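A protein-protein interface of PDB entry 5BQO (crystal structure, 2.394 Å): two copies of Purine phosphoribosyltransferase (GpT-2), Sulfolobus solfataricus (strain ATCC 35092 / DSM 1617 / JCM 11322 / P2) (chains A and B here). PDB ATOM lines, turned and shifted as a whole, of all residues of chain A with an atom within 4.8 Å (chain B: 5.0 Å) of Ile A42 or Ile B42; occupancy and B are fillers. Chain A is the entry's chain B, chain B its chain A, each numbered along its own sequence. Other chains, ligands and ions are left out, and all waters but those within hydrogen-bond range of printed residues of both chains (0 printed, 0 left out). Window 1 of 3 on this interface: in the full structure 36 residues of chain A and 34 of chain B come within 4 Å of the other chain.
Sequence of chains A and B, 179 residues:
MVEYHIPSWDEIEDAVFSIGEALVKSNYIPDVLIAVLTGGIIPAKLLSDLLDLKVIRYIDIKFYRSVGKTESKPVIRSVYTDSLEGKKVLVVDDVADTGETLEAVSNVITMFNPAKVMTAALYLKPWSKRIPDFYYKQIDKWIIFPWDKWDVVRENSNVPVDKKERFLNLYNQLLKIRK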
ATOM      1  N   TRP A   9      18.007  -6.971   9.817  1.00  0.00           N
ATOM      2  CA  TRP A   9      18.227  -7.604   8.522  1.00  0.00           C
ATOM      3  C   TRP A   9      19.137  -8.817   8.678  1.00  0.00           C
ATOM      4  O   TRP A   9      19.044  -9.784   7.920  1.00  0.00           O
ATOM      5  CB  TRP A   9      18.840  -6.614   7.528  1.00  0.00           C
ATOM      6  CG  TRP A   9      17.860  -5.657   6.917  1.00  0.00           C
ATOM      7  CD1 TRP A   9      17.739  -4.325   7.185  1.00  0.00           C
ATOM      8  CD2 TRP A   9      16.872  -5.957   5.923  1.00  0.00           C
ATOM      9  NE1 TRP A   9      16.736  -3.777   6.422  1.00  0.00           N
ATOM     10  CE2 TRP A   9      16.187  -4.758   5.639  1.00  0.00           C
ATOM     11  CE3 TRP A   9      16.497  -7.122   5.247  1.00  0.00           C
ATOM     12  CZ2 TRP A   9      15.152  -4.690   4.709  1.00  0.00           C
ATOM     13  CZ3 TRP A   9      15.466  -7.055   4.326  1.00  0.00           C
ATOM     14  CH2 TRP A   9      14.806  -5.846   4.066  1.00  0.00           C
ATOM     15  N   GLY A  39       3.976  -9.770   1.927  1.00  0.00           N
ATOM     16  CA  GLY A  39       4.824  -9.950   3.092  1.00  0.00           C
ATOM     17  C   GLY A  39       5.920 -10.980   2.903  1.00  0.00           C
ATOM     18  O   GLY A  39       6.966 -10.908   3.549  1.00  0.00           O
ATOM     19  N   GLY A  40       5.691 -11.938   2.011  1.00  0.00           N
ATOM     20  CA  GLY A  40       6.629 -13.028   1.816  1.00  0.00           C
ATOM     21  C   GLY A  40       7.497 -12.910   0.577  1.00  0.00           C
ATOM     22  O   GLY A  40       8.267 -13.819   0.269  1.00  0.00           O
ATOM     23  N   ILE A  41       7.389 -11.789  -0.129  1.00  0.00           N
ATOM     24  CA  ILE A  41       8.101 -11.620  -1.391  1.00  0.00           C
ATOM     25  C   ILE A  41       9.588 -11.322  -1.179  1.00  0.00           C
ATOM     26  O   ILE A  41      10.399 -11.497  -2.089  1.00  0.00           O
ATOM     27  CB  ILE A  41       7.469 -10.500  -2.247  1.00  0.00           C
ATOM     28  CG1 ILE A  41       7.790 -10.716  -3.729  1.00  0.00           C
ATOM     29  CG2 ILE A  41       7.918  -9.125  -1.767  1.00  0.00           C
ATOM     30  CD1 ILE A  41       7.231  -9.648  -4.641  1.00  0.00           C
ATOM     31  N   ILE A  42       9.948 -10.877   0.021  1.00  0.00           N
ATOM     32  CA  ILE A  42      11.354 -10.662   0.357  1.00  0.00           C
ATOM     33  C   ILE A  42      12.007 -11.943   0.909  1.00  0.00           C
ATOM     34  O   ILE A  42      13.144 -12.252   0.547  1.00  0.00           O
ATOM     35  CB  ILE A  42      11.531  -9.494   1.364  1.00  0.00           C
ATOM     36  CG1 ILE A  42      11.178  -8.160   0.700  1.00  0.00           C
ATOM     37  CG2 ILE A  42      12.955  -9.445   1.897  1.00  0.00           C
ATOM     38  CD1 ILE A  42      11.556  -6.946   1.523  1.00  0.00           C
ATOM     39  N   PRO A  43      11.303 -12.698   1.781  1.00  0.00           N
ATOM     40  CA  PRO A  43      11.875 -14.003   2.136  1.00  0.00           C
ATOM     41  C   PRO A  43      12.025 -14.946   0.940  1.00  0.00           C
ATOM     42  O   PRO A  43      13.020 -15.669   0.858  1.00  0.00           O
ATOM     43  CB  PRO A  43      10.862 -14.566   3.136  1.00  0.00           C
ATOM     44  CG  PRO A  43      10.250 -13.371   3.752  1.00  0.00           C
ATOM     45  CD  PRO A  43      10.162 -12.356   2.653  1.00  0.00           C
ATOM     46  N   ALA A  44      11.052 -14.936   0.034  1.00  0.00           N
ATOM     47  CA  ALA A  44      11.083 -15.806  -1.138  1.00  0.00           C
ATOM     48  C   ALA A  44      12.277 -15.491  -2.033  1.00  0.00           C
ATOM     49  O   ALA A  44      12.957 -16.397  -2.512  1.00  0.00           O
ATOM     50  CB  ALA A  44       9.788 -15.682  -1.924  1.00  0.00           C
ATOM     51  N   LYS A  45      12.524 -14.204  -2.251  1.00  0.00           N
ATOM     52  CA  LYS A  45      13.639 -13.759  -3.080  1.00  0.00           C
ATOM     53  C   LYS A  45      14.984 -14.157  -2.475  1.00  0.00           C
ATOM     54  O   LYS A  45      15.886 -14.607  -3.182  1.00  0.00           O
ATOM     55  CB  LYS A  45      13.576 -12.241  -3.278  1.00  0.00           C
ATOM     56  CG  LYS A  45      14.833 -11.624  -3.875  1.00  0.00           C
ATOM     57  CD  LYS A  45      15.116 -12.149  -5.273  1.00  0.00           C
ATOM     58  CE  LYS A  45      16.404 -11.560  -5.826  1.00  0.00           C
ATOM     59  NZ  LYS A  45      16.790 -12.168  -7.128  1.00  0.00           N
ATOM     60  N   LEU A  46      15.108 -13.991  -1.162  1.00  0.00           N
ATOM     61  CA  LEU A  46      16.349 -14.306  -0.464  1.00  0.00           C
ATOM     62  C   LEU A  46      16.599 -15.810  -0.409  1.00  0.00           C
ATOM     63  O   LEU A  46      17.732 -16.261  -0.572  1.00  0.00           O
ATOM     64  CB  LEU A  46      16.328 -13.722   0.949  1.00  0.00           C
ATOM     65  CG  LEU A  46      16.390 -12.195   1.028  1.00  0.00           C
ATOM     66  CD1 LEU A  46      16.164 -11.717   2.454  1.00  0.00           C
ATOM     67  CD2 LEU A  46      17.719 -11.687   0.491  1.00  0.00           C
ATOM     68  N   TRP A 147      10.283  -4.495   6.305  1.00  0.00           N
ATOM     69  CA  TRP A 147       9.526  -4.099   5.120  1.00  0.00           C
ATOM     70  C   TRP A 147       8.092  -3.674   5.430  1.00  0.00           C
ATOM     71  O   TRP A 147       7.278  -3.522   4.519  1.00  0.00           O
ATOM     72  CB  TRP A 147       9.516  -5.234   4.091  1.00  0.00           C
ATOM     73  CG  TRP A 147       9.251  -6.591   4.667  1.00  0.00           C
ATOM     74  CD1 TRP A 147       8.032  -7.143   4.937  1.00  0.00           C
ATOM     75  CD2 TRP A 147      10.227  -7.574   5.031  1.00  0.00           C
ATOM     76  NE1 TRP A 147       8.191  -8.407   5.453  1.00  0.00           N
ATOM     77  CE2 TRP A 147       9.529  -8.696   5.519  1.00  0.00           C
ATOM     78  CE3 TRP A 147      11.624  -7.614   4.994  1.00  0.00           C
ATOM     79  CZ2 TRP A 147      10.179  -9.844   5.966  1.00  0.00           C
ATOM     80  CZ3 TRP A 147      12.268  -8.755   5.437  1.00  0.00           C
ATOM     81  CH2 TRP A 147      11.545  -9.854   5.918  1.00  0.00           C
ATOM     82  N   TRP B   9      22.541  -3.409   3.944  1.00  0.00           N
ATOM     83  CA  TRP B   9      21.102  -3.183   4.002  1.00  0.00           C
ATOM     84  C   TRP B   9      20.816  -1.746   4.423  1.00  0.00           C
ATOM     85  O   TRP B   9      19.842  -1.138   3.980  1.00  0.00           O
ATOM     86  CB  TRP B   9      20.433  -4.158   4.972  1.00  0.00           C
ATOM     87  CG  TRP B   9      20.252  -5.540   4.428  1.00  0.00           C
ATOM     88  CD1 TRP B   9      20.963  -6.653   4.766  1.00  0.00           C
ATOM     89  CD2 TRP B   9      19.291  -5.959   3.451  1.00  0.00           C
ATOM     90  NE1 TRP B   9      20.506  -7.741   4.062  1.00  0.00           N
ATOM     91  CE2 TRP B   9      19.478  -7.340   3.246  1.00  0.00           C
ATOM     92  CE3 TRP B   9      18.290  -5.301   2.729  1.00  0.00           C
ATOM     93  CZ2 TRP B   9      18.702  -8.076   2.352  1.00  0.00           C
ATOM     94  CZ3 TRP B   9      17.522  -6.033   1.839  1.00  0.00           C
ATOM     95  CH2 TRP B   9      17.733  -7.405   1.659  1.00  0.00           C
ATOM     96  N   THR B  38      13.613 -10.224 -11.091  1.00  0.00           N
ATOM     97  CA  THR B  38      13.299 -10.272  -9.666  1.00  0.00           C
ATOM     98  C   THR B  38      14.131  -9.278  -8.861  1.00  0.00           C
ATOM     99  O   THR B  38      14.026  -9.218  -7.635  1.00  0.00           O
ATOM    100  CB  THR B  38      13.527 -11.682  -9.093  1.00  0.00           C
ATOM    101  OG1 THR B  38      14.903 -12.048  -9.254  1.00  0.00           O
ATOM    102  CG2 THR B  38      12.651 -12.697  -9.810  1.00  0.00           C
ATOM    103  N   GLY B  39      14.956  -8.501  -9.552  1.00  0.00           N
ATOM    104  CA  GLY B  39      15.839  -7.554  -8.895  1.00  0.00           C
ATOM    105  C   GLY B  39      15.112  -6.372  -8.283  1.00  0.00           C
ATOM    106  O   GLY B  39      15.596  -5.761  -7.332  1.00  0.00           O
ATOM    107  N   GLY B  40      13.943  -6.051  -8.829  1.00  0.00           N
ATOM    108  CA  GLY B  40      13.168  -4.922  -8.351  1.00  0.00           C
ATOM    109  C   GLY B  40      12.205  -5.291  -7.239  1.00  0.00           C
ATOM    110  O   GLY B  40      11.551  -4.420  -6.668  1.00  0.00           O
ATOM    111  N   ILE B  41      12.126  -6.584  -6.937  1.00  0.00           N
ATOM    112  CA  ILE B  41      11.230  -7.102  -5.905  1.00  0.00           C
ATOM    113  C   ILE B  41      11.385  -6.378  -4.571  1.00  0.00           C
ATOM    114  O   ILE B  41      10.425  -5.824  -4.037  1.00  0.00           O
ATOM    115  CB  ILE B  41      11.464  -8.611  -5.672  1.00  0.00           C
ATOM    116  CG1 ILE B  41      10.856  -9.429  -6.811  1.00  0.00           C
ATOM    117  CG2 ILE B  41      10.873  -9.052  -4.342  1.00  0.00           C
ATOM    118  CD1 ILE B  41      10.964 -10.924  -6.606  1.00  0.00           C
ATOM    119  N   ILE B  42      12.604  -6.380  -4.044  1.00  0.00           N
ATOM    120  CA  ILE B  42      12.868  -5.829  -2.721  1.00  0.00           C
ATOM    121  C   ILE B  42      12.835  -4.290  -2.672  1.00  0.00           C
ATOM    122  O   ILE B  42      12.289  -3.728  -1.723  1.00  0.00           O
ATOM    123  CB  ILE B  42      14.221  -6.347  -2.180  1.00  0.00           C
ATOM    124  CG1 ILE B  42      14.189  -7.876  -2.096  1.00  0.00           C
ATOM    125  CG2 ILE B  42      14.534  -5.738  -0.822  1.00  0.00           C
ATOM    126  CD1 ILE B  42      15.300  -8.477  -1.272  1.00  0.00           C
ATOM    127  N   PRO B  43      13.408  -3.601  -3.680  1.00  0.00           N
ATOM    128  CA  PRO B  43      13.256  -2.140  -3.645  1.00  0.00           C
ATOM    129  C   PRO B  43      11.800  -1.676  -3.728  1.00  0.00           C
ATOM    130  O   PRO B  43      11.420  -0.746  -3.014  1.00  0.00           O
ATOM    131  CB  PRO B  43      14.035  -1.677  -4.878  1.00  0.00           C
ATOM    132  CG  PRO B  43      15.043  -2.739  -5.102  1.00  0.00           C
ATOM    133  CD  PRO B  43      14.353  -4.018  -4.735  1.00  0.00           C
ATOM    134  N   ALA B  44      11.004  -2.314  -4.582  1.00  0.00           N
ATOM    135  CA  ALA B  44       9.606  -1.929  -4.769  1.00  0.00           C
ATOM    136  C   ALA B  44       8.804  -2.076  -3.481  1.00  0.00           C
ATOM    137  O   ALA B  44       7.994  -1.213  -3.144  1.00  0.00           O
ATOM    138  CB  ALA B  44       8.972  -2.754  -5.879  1.00  0.00           C
ATOM    139  N   LYS B  45       9.033  -3.173  -2.767  1.00  0.00           N
ATOM    140  CA  LYS B  45       8.346  -3.430  -1.505  1.00  0.00           C
ATOM    141  C   LYS B  45       8.702  -2.383  -0.453  1.00  0.00           C
ATOM    142  O   LYS B  45       7.827  -1.876   0.250  1.00  0.00           O
ATOM    143  CB  LYS B  45       8.683  -4.831  -0.989  1.00  0.00           C
ATOM    144  CG  LYS B  45       8.201  -5.109   0.427  1.00  0.00           C
ATOM    145  CD  LYS B  45       6.686  -5.030   0.531  1.00  0.00           C
ATOM    146  CE  LYS B  45       6.216  -5.346   1.943  1.00  0.00           C
ATOM    147  NZ  LYS B  45       4.757  -5.107   2.111  1.00  0.00           N
ATOM    148  N   LEU B  46       9.990  -2.066  -0.351  1.00  0.00           N
ATOM    149  CA  LEU B  46      10.461  -1.072   0.608  1.00  0.00           C
ATOM    150  C   LEU B  46       9.906   0.311   0.290  1.00  0.00           C
ATOM    151  O   LEU B  46       9.458   1.028   1.185  1.00  0.00           O
ATOM    152  CB  LEU B  46      11.990  -1.028   0.632  1.00  0.00           C
ATOM    153  CG  LEU B  46      12.705  -2.287   1.125  1.00  0.00           C
ATOM    154  CD1 LEU B  46      14.211  -2.075   1.131  1.00  0.00           C
ATOM    155  CD2 LEU B  46      12.208  -2.685   2.507  1.00  0.00           C
ATOM    156  N   TRP B 147      20.574  -9.451  -2.104  1.00  0.00           N
ATOM    157  CA  TRP B 147      19.634 -10.460  -2.587  1.00  0.00           C
ATOM    158  C   TRP B 147      20.133 -11.225  -3.813  1.00  0.00           C
ATOM    159  O   TRP B 147      19.367 -11.948  -4.449  1.00  0.00           O
ATOM    160  CB  TRP B 147      18.277  -9.821  -2.899  1.00  0.00           C
ATOM    161  CG  TRP B 147      18.347  -8.523  -3.649  1.00  0.00           C
ATOM    162  CD1 TRP B 147      18.422  -8.359  -5.002  1.00  0.00           C
ATOM    163  CD2 TRP B 147      18.324  -7.205  -3.086  1.00  0.00           C
ATOM    164  NE1 TRP B 147      18.459  -7.020  -5.316  1.00  0.00           N
ATOM    165  CE2 TRP B 147      18.400  -6.291  -4.156  1.00  0.00           C
ATOM    166  CE3 TRP B 147      18.255  -6.709  -1.780  1.00  0.00           C
ATOM    167  CZ2 TRP B 147      18.406  -4.912  -3.961  1.00  0.00           C
ATOM    168  CZ3 TRP B 147      18.260  -5.340  -1.589  1.00  0.00           C
ATOM    169  CH2 TRP B 147      18.336  -4.457  -2.674  1.00  0.00           C
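The side-chain hydroxyl (OG1) of Thr B38 sits at hydrogen-bond distance from the side-chain amino group (NZ) of Lys A45 (2.8 Å).
O of Gly A39 sits at hydrogen-bond distance from NE1 of Trp A147 (3.4 Å).
Trp A9 touches Trp B9 (CZ3 to CZ3, 3.4 Å). O of Ile A41 touches CG2 of Ile B41 (3.4 Å). CD1 of Ile A42 touches CG2 of Ile B42, at 3.98 Å. Lys B45 touches Ile A42. O of Trp B147 touches CE of Lys A45 (3.3 Å). Leu A46 touches Trp B147 (CD2 to CA, 3.8 Å). Lys B45 touches Trp A147.
Gly A39 touches none of the printed residues of chain B. Of chain B, only Ile B42 (3.98 Å) and Lys B45 (3.98 Å) come within 4 Å of Ile A42. Printed residues of chain A within 4 Å of Ile B41: Ile A41 (3.4 Å). Ile B42 touches just one residue of chain A: Ile A42 (3.98 Å). Ala B44 touches none of the printed residues of chain A. Of the printed residues of chain A, Lys B45 touches Ile A42 (3.98 Å) and Trp A147 (3.3 Å). The nearest residue of chain A that does not touch Ile B42 is Lys A45 (4.1 Å).
Of the 11 printed residues of chain B, 6 touch a printed residue of chain A. Printed residues of chain A that touch a printed residue of chain B: Trp A9, Ile A41, Ile A42, Lys A45, Leu A46 and Trp A147.
Ile B41 touches its own counterpart, Ile A41. Ile A42 touches Lys B45, but with the chains exchanged Lys A45 does not touch Ile B42 (4.1 Å). Lys A45 touches Trp B147, and with the chains exchanged Trp A147 touches Lys B45. Leu A46 touches Trp B147, but with the chains exchanged Trp A147 does not touch Leu B46 (4.003 Å). Positions printed for both chains: 9, 39, 40, 41, 42, 43, 44, 45, 46 and 147. Of the 8 pairs that touch across the chains among the printed residues, 5 have their exchanged pair printed and touching as well.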
